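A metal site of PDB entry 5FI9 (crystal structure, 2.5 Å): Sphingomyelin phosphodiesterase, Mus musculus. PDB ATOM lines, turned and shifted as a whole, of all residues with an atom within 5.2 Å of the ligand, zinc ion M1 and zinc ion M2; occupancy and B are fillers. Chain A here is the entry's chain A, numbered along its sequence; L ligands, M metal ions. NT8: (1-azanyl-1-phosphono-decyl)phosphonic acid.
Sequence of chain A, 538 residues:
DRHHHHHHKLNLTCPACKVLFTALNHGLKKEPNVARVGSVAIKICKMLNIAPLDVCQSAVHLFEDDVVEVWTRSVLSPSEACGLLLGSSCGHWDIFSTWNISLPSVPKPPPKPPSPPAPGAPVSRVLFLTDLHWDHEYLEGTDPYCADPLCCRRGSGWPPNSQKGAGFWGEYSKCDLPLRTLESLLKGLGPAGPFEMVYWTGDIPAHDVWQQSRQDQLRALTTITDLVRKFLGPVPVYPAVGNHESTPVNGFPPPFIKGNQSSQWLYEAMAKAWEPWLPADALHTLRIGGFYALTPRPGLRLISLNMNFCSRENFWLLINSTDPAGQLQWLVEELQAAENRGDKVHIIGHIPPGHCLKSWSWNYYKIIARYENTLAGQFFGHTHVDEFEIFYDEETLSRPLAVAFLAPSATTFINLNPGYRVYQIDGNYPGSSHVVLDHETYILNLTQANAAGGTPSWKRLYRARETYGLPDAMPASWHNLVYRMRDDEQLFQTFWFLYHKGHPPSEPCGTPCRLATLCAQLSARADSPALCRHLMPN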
ATOM      1  N   ASP A 131     -11.336   0.881  13.764  1.00  0.00           N
ATOM      2  CA  ASP A 131     -10.358   1.554  12.913  1.00  0.00           C
ATOM      3  C   ASP A 131     -11.042   2.445  11.885  1.00  0.00           C
ATOM      4  O   ASP A 131     -10.811   2.347  10.680  1.00  0.00           O
ATOM      5  CB  ASP A 131      -9.451   0.522  12.227  1.00  0.00           C
ATOM      6  CG  ASP A 131      -8.758  -0.399  13.221  1.00  0.00           C
ATOM      7  OD1 ASP A 131      -7.632  -0.081  13.643  1.00  0.00           O
ATOM      8  OD2 ASP A 131      -9.361  -1.441  13.582  1.00  0.00           O
ATOM      9  N   HIS A 133     -10.677   5.794  11.842  1.00  0.00           N
ATOM     10  CA  HIS A 133      -9.591   6.698  11.459  1.00  0.00           C
ATOM     11  C   HIS A 133     -10.111   7.854  10.598  1.00  0.00           C
ATOM     12  O   HIS A 133      -9.834   7.956   9.403  1.00  0.00           O
ATOM     13  CB  HIS A 133      -8.485   5.927  10.722  1.00  0.00           C
ATOM     14  CG  HIS A 133      -7.748   4.947  11.588  1.00  0.00           C
ATOM     15  ND1 HIS A 133      -6.861   5.352  12.557  1.00  0.00           N
ATOM     16  CD2 HIS A 133      -7.753   3.600  11.621  1.00  0.00           C
ATOM     17  CE1 HIS A 133      -6.353   4.284  13.155  1.00  0.00           C
ATOM     18  NE2 HIS A 133      -6.876   3.204  12.604  1.00  0.00           N
ATOM     19  N   ASP A 203      -9.520   3.381  17.767  1.00  0.00           N
ATOM     20  CA  ASP A 203      -8.784   3.964  16.643  1.00  0.00           C
ATOM     21  C   ASP A 203      -9.690   4.900  15.833  1.00  0.00           C
ATOM     22  O   ASP A 203     -10.078   4.626  14.700  1.00  0.00           O
ATOM     23  CB  ASP A 203      -8.158   2.869  15.768  1.00  0.00           C
ATOM     24  CG  ASP A 203      -6.739   2.533  16.170  1.00  0.00           C
ATOM     25  OD1 ASP A 203      -6.042   1.828  15.404  1.00  0.00           O
ATOM     26  OD2 ASP A 203      -6.307   2.983  17.260  1.00  0.00           O
ATOM     27  N   HIS A 207      -4.002   9.088  11.235  1.00  0.00           N
ATOM     28  CA  HIS A 207      -2.591   8.857  11.515  1.00  0.00           C
ATOM     29  C   HIS A 207      -1.749  10.119  11.390  1.00  0.00           C
ATOM     30  O   HIS A 207      -0.531  10.018  11.178  1.00  0.00           O
ATOM     31  CB  HIS A 207      -2.048   7.767  10.592  1.00  0.00           C
ATOM     32  CG  HIS A 207      -2.804   6.476  10.678  1.00  0.00           C
ATOM     33  ND1 HIS A 207      -4.088   6.323  10.190  1.00  0.00           N
ATOM     34  CD2 HIS A 207      -2.451   5.267  11.179  1.00  0.00           C
ATOM     35  CE1 HIS A 207      -4.493   5.083  10.398  1.00  0.00           C
ATOM     36  NE2 HIS A 207      -3.515   4.423  11.003  1.00  0.00           N
ATOM     37  N   ASN A 243      -5.272   2.589  20.221  1.00  0.00           N
ATOM     38  CA  ASN A 243      -3.946   3.123  20.472  1.00  0.00           C
ATOM     39  C   ASN A 243      -3.715   4.501  19.873  1.00  0.00           C
ATOM     40  O   ASN A 243      -2.748   5.167  20.253  1.00  0.00           O
ATOM     41  CB  ASN A 243      -2.875   2.154  19.945  1.00  0.00           C
ATOM     42  CG  ASN A 243      -3.032   1.861  18.463  1.00  0.00           C
ATOM     43  OD1 ASN A 243      -4.123   1.576  17.985  1.00  0.00           O
ATOM     44  ND2 ASN A 243      -1.924   1.942  17.732  1.00  0.00           N
ATOM     45  N   HIS A 244      -4.582   4.952  18.968  1.00  0.00           N
ATOM     46  CA  HIS A 244      -4.472   6.292  18.389  1.00  0.00           C
ATOM     47  C   HIS A 244      -5.281   7.332  19.136  1.00  0.00           C
ATOM     48  O   HIS A 244      -5.186   8.529  18.818  1.00  0.00           O
ATOM     49  CB  HIS A 244      -4.907   6.270  16.922  1.00  0.00           C
ATOM     50  CG  HIS A 244      -3.903   5.677  15.989  1.00  0.00           C
ATOM     51  ND1 HIS A 244      -2.992   6.438  15.295  1.00  0.00           N
ATOM     52  CD2 HIS A 244      -3.663   4.392  15.634  1.00  0.00           C
ATOM     53  CE1 HIS A 244      -2.228   5.654  14.550  1.00  0.00           C
ATOM     54  NE2 HIS A 244      -2.623   4.404  14.732  1.00  0.00           N
ATOM     55  N   HIS A 350      -8.786  -3.651  21.334  1.00  0.00           N
ATOM     56  CA  HIS A 350      -8.296  -3.123  20.070  1.00  0.00           C
ATOM     57  C   HIS A 350      -7.157  -3.981  19.528  1.00  0.00           C
ATOM     58  O   HIS A 350      -7.319  -4.679  18.526  1.00  0.00           O
ATOM     59  CB  HIS A 350      -7.834  -1.676  20.224  1.00  0.00           C
ATOM     60  CG  HIS A 350      -7.321  -1.094  18.952  1.00  0.00           C
ATOM     61  ND1 HIS A 350      -8.122  -0.904  17.844  1.00  0.00           N
ATOM     62  CD2 HIS A 350      -6.087  -0.672  18.600  1.00  0.00           C
ATOM     63  CE1 HIS A 350      -7.406  -0.389  16.862  1.00  0.00           C
ATOM     64  NE2 HIS A 350      -6.163  -0.235  17.291  1.00  0.00           N
ATOM     65  N   HIS A 382      -7.364  -3.504  14.807  1.00  0.00           N
ATOM     66  CA  HIS A 382      -5.978  -3.021  14.832  1.00  0.00           C
ATOM     67  C   HIS A 382      -5.175  -3.475  13.611  1.00  0.00           C
ATOM     68  O   HIS A 382      -4.309  -2.732  13.133  1.00  0.00           O
ATOM     69  CB  HIS A 382      -5.287  -3.483  16.118  1.00  0.00           C
ATOM     70  CG  HIS A 382      -3.944  -2.856  16.338  1.00  0.00           C
ATOM     71  ND1 HIS A 382      -3.773  -1.486  16.456  1.00  0.00           N
ATOM     72  CD2 HIS A 382      -2.715  -3.406  16.490  1.00  0.00           C
ATOM     73  CE1 HIS A 382      -2.494  -1.236  16.653  1.00  0.00           C
ATOM     74  NE2 HIS A 382      -1.830  -2.376  16.676  1.00  0.00           N
ATOM     75  N   THR A 383      -5.448  -4.676  13.096  1.00  0.00           N
ATOM     76  CA  THR A 383      -4.712  -5.159  11.935  1.00  0.00           C
ATOM     77  C   THR A 383      -5.229  -4.568  10.625  1.00  0.00           C
ATOM     78  O   THR A 383      -4.492  -4.557   9.638  1.00  0.00           O
ATOM     79  CB  THR A 383      -4.799  -6.686  11.851  1.00  0.00           C
ATOM     80  OG1 THR A 383      -6.163  -7.090  11.692  1.00  0.00           O
ATOM     81  CG2 THR A 383      -4.226  -7.320  13.105  1.00  0.00           C
ATOM     82  N   HIS A 384      -6.480  -4.098  10.606  1.00  0.00           N
ATOM     83  CA  HIS A 384      -7.132  -3.502   9.452  1.00  0.00           C
ATOM     84  C   HIS A 384      -7.452  -4.522   8.366  1.00  0.00           C
ATOM     85  O   HIS A 384      -7.953  -4.132   7.298  1.00  0.00           O
ATOM     86  CB  HIS A 384      -6.312  -2.356   8.836  1.00  0.00           C
ATOM     87  CG  HIS A 384      -6.126  -1.182   9.745  1.00  0.00           C
ATOM     88  ND1 HIS A 384      -5.892   0.091   9.281  1.00  0.00           N
ATOM     89  CD2 HIS A 384      -6.157  -1.086  11.098  1.00  0.00           C
ATOM     90  CE1 HIS A 384      -5.774   0.925  10.300  1.00  0.00           C
ATOM     91  NE2 HIS A 384      -5.931   0.230  11.419  1.00  0.00           N
ATOM     92  N   VAL A 385      -7.198  -5.810   8.589  1.00  0.00           N
ATOM     93  CA  VAL A 385      -7.485  -6.861   7.624  1.00  0.00           C
ATOM     94  C   VAL A 385      -8.349  -7.919   8.309  1.00  0.00           C
ATOM     95  O   VAL A 385      -8.499  -7.929   9.532  1.00  0.00           O
ATOM     96  CB  VAL A 385      -6.205  -7.486   7.041  1.00  0.00           C
ATOM     97  CG1 VAL A 385      -5.553  -6.535   6.048  1.00  0.00           C
ATOM     98  CG2 VAL A 385      -5.224  -7.849   8.148  1.00  0.00           C
ATOM     99  N   PHE A 413      -6.512   2.899   4.895  1.00  0.00           N
ATOM    100  CA  PHE A 413      -5.149   2.690   5.376  1.00  0.00           C
ATOM    101  C   PHE A 413      -4.840   1.197   5.585  1.00  0.00           C
ATOM    102  O   PHE A 413      -5.374   0.618   6.530  1.00  0.00           O
ATOM    103  CB  PHE A 413      -4.974   3.464   6.689  1.00  0.00           C
ATOM    104  CG  PHE A 413      -3.547   3.825   7.001  1.00  0.00           C
ATOM    105  CD1 PHE A 413      -2.985   4.974   6.479  1.00  0.00           C
ATOM    106  CD2 PHE A 413      -2.785   3.029   7.832  1.00  0.00           C
ATOM    107  CE1 PHE A 413      -1.678   5.315   6.774  1.00  0.00           C
ATOM    108  CE2 PHE A 413      -1.485   3.359   8.133  1.00  0.00           C
ATOM    109  CZ  PHE A 413      -0.928   4.507   7.601  1.00  0.00           C
ATOM    110  N   ILE A 414      -4.012   0.551   4.758  1.00  0.00           N
ATOM    111  CA  ILE A 414      -3.372   1.105   3.550  1.00  0.00           C
ATOM    112  C   ILE A 414      -3.776   0.269   2.348  1.00  0.00           C
ATOM    113  O   ILE A 414      -3.732  -0.958   2.398  1.00  0.00           O
ATOM    114  CB  ILE A 414      -1.830   1.121   3.690  1.00  0.00           C
ATOM    115  CG1 ILE A 414      -1.396   2.031   4.834  1.00  0.00           C
ATOM    116  CG2 ILE A 414      -1.170   1.573   2.383  1.00  0.00           C
ATOM    117  CD1 ILE A 414      -0.088   1.607   5.482  1.00  0.00           C
ATOM    118  N   LEU A 416      -6.590  -0.459   0.962  1.00  0.00           N
ATOM    119  CA  LEU A 416      -7.680  -1.367   1.269  1.00  0.00           C
ATOM    120  C   LEU A 416      -9.006  -0.699   0.937  1.00  0.00           C
ATOM    121  O   LEU A 416      -9.090   0.516   0.762  1.00  0.00           O
ATOM    122  CB  LEU A 416      -7.675  -1.777   2.756  1.00  0.00           C
ATOM    123  CG  LEU A 416      -6.510  -2.626   3.234  1.00  0.00           C
ATOM    124  CD1 LEU A 416      -6.439  -2.618   4.760  1.00  0.00           C
ATOM    125  CD2 LEU A 416      -6.631  -4.046   2.716  1.00  0.00           C
ATOM    126  N   TYR A 499      -8.976 -11.318   2.902  1.00  0.00           N
ATOM    127  CA  TYR A 499      -8.015 -10.730   3.823  1.00  0.00           C
ATOM    128  C   TYR A 499      -7.918  -9.224   3.635  1.00  0.00           C
ATOM    129  O   TYR A 499      -7.967  -8.459   4.599  1.00  0.00           O
ATOM    130  CB  TYR A 499      -6.653 -11.397   3.608  1.00  0.00           C
ATOM    131  CG  TYR A 499      -5.579 -11.091   4.631  1.00  0.00           C
ATOM    132  CD1 TYR A 499      -5.376 -11.912   5.733  1.00  0.00           C
ATOM    133  CD2 TYR A 499      -4.743  -9.993   4.473  1.00  0.00           C
ATOM    134  CE1 TYR A 499      -4.381 -11.653   6.655  1.00  0.00           C
ATOM    135  CE2 TYR A 499      -3.746  -9.714   5.403  1.00  0.00           C
ATOM    136  CZ  TYR A 499      -3.565 -10.550   6.483  1.00  0.00           C
ATOM    137  OH  TYR A 499      -2.584 -10.283   7.401  1.00  0.00           O
ATOM    138  N   HIS A 500      -7.799  -8.785   2.375  1.00  0.00           N
ATOM    139  CA  HIS A 500      -7.658  -7.368   2.052  1.00  0.00           C
ATOM    140  C   HIS A 500      -8.977  -6.723   1.640  1.00  0.00           C
ATOM    141  O   HIS A 500      -8.975  -5.710   0.942  1.00  0.00           O
ATOM    142  CB  HIS A 500      -6.623  -7.194   0.941  1.00  0.00           C
ATOM    143  CG  HIS A 500      -5.315  -7.867   1.214  1.00  0.00           C
ATOM    144  ND1 HIS A 500      -4.220  -7.196   1.711  1.00  0.00           N
ATOM    145  CD2 HIS A 500      -4.931  -9.161   1.070  1.00  0.00           C
ATOM    146  CE1 HIS A 500      -3.214  -8.034   1.863  1.00  0.00           C
ATOM    147  NE2 HIS A 500      -3.620  -9.240   1.483  1.00  0.00           N
HETATM  148  N01 NT8 L   1      -1.697  -1.107  13.284  1.00  0.00           N
HETATM  149  C02 NT8 L   1      -1.898   0.230  12.848  1.00  0.00           C
HETATM  150  C03 NT8 L   1      -2.180   0.272  11.365  1.00  0.00           C
HETATM  151  C04 NT8 L   1      -1.801  -0.998  10.647  1.00  0.00           C
HETATM  152  C05 NT8 L   1      -1.816  -0.813   9.148  1.00  0.00           C
HETATM  153  C06 NT8 L   1      -2.117  -2.109   8.423  1.00  0.00           C
HETATM  154  C07 NT8 L   1      -2.075  -1.946   6.920  1.00  0.00           C
HETATM  155  C08 NT8 L   1      -2.634  -3.150   6.201  1.00  0.00           C
HETATM  156  C09 NT8 L   1      -1.581  -3.851   5.379  1.00  0.00           C
HETATM  157  C10 NT8 L   1      -2.160  -4.992   4.572  1.00  0.00           C
HETATM  158  C11 NT8 L   1      -2.357  -4.600   3.127  1.00  0.00           C
HETATM  159  P12 NT8 L   1      -3.276   0.985  13.757  1.00  0.00           P
HETATM  160  O13 NT8 L   1      -3.699   2.256  13.070  1.00  0.00           O
HETATM  161  O14 NT8 L   1      -2.835   1.310  15.161  1.00  0.00           O
HETATM  162  O15 NT8 L   1      -4.431   0.014  13.789  1.00  0.00           O
HETATM  163  P16 NT8 L   1      -0.395   1.201  13.183  1.00  0.00           P
HETATM  164  O17 NT8 L   1       0.169   0.802  14.524  1.00  0.00           O
HETATM  165  O18 NT8 L   1      -0.749   2.676  13.189  1.00  0.00           O
HETATM  166  O19 NT8 L   1       0.624   0.939  12.100  1.00  0.00           O
HETATM  167 ZN    ZN M   1      -4.556   0.488  16.244  1.00  0.00          ZN
HETATM  168 ZN    ZN M   2      -6.245   1.354  13.191  1.00  0.00          ZN
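Of the 16 residues printed, 4 come within 4 Å of zinc ion M2.
The nearest printed residue that does not touch zinc ion M2 is His 350 (4.2 Å).
Within 4 Å of zinc ion M1: Asp 203, Asn 243, His 350 and His 382.
The nearest printed residue that does not touch zinc ion M1 is His 244 (4.1 Å).
O of Thr 383 touches C06 of the ligand, 3.6 Å away.
N of Ile 414 touches C07 of the ligand, at 3.8 Å.
ND1 of His 500 touches C11 of the ligand (3.5 Å).
Hydrophobic or aromatic side chains within 4 Å of the ligand: His 133, His 207, His 244, His 382, His 384 and His 500.
Within 4 Å of the ligand: Asp 131, His 133, Asp 203, His 207, Asn 243, His 244, His 350, His 382, Thr 383, His 384, Ile 414 and His 500.
N01 of the ligand is in hydrogen-bond range of O of His 382, 3.1 Å away.
NE2 of His 244 sits at hydrogen-bond distance from O13 of the ligand, at 2.9 Å.
NE2 of His 207 sits at hydrogen-bond distance from O13 of the ligand (3.0 Å).
Zinc ion M1 is bound by a ring nitrogen (NE2) of His 350 (2.0 Å), the side-chain amide oxygen (OD1) of Asn 243 (2.1 Å), a ring nitrogen (ND1) of His 382 (2.1 Å), the side-chain carboxylate (OD1) of Asp 203 (2.2 Å), an oxygen (O14) of the ligand (2.2 Å) and an oxygen (O15) of the ligand (2.5 Å).
Zinc ion M1 has six donor atoms within binding distance.
OD2 of Asp 131 lies within hydrogen-bond range of N of His 382 (3.1 Å).
The side-chain carboxylate of Asp 203 sits at hydrogen-bond distance from the backbone NH of His 244 (3.1 Å).
The side-chain hydroxyl (OG1) of Thr 383 is in hydrogen-bond range of the backbone carbonyl oxygen (O) of Val 385 (3.3 Å).
ND1 of His 384 lies within hydrogen-bond range of O of Phe 413 (2.8 Å).
Zinc ion M2 is bound by a ring nitrogen (NE2) of His 133 (2.0 Å), the side-chain carboxylate of Asp 131 (2.0 Å), a ring nitrogen (NE2) of His 384 (2.1 Å), the side-chain carboxylate of Asp 203 (2.3 Å) and an oxygen (O15) of the ligand (2.3 Å).
Slightly farther from zinc ion M2 lies an oxygen (O13) of the ligand (2.7 Å).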
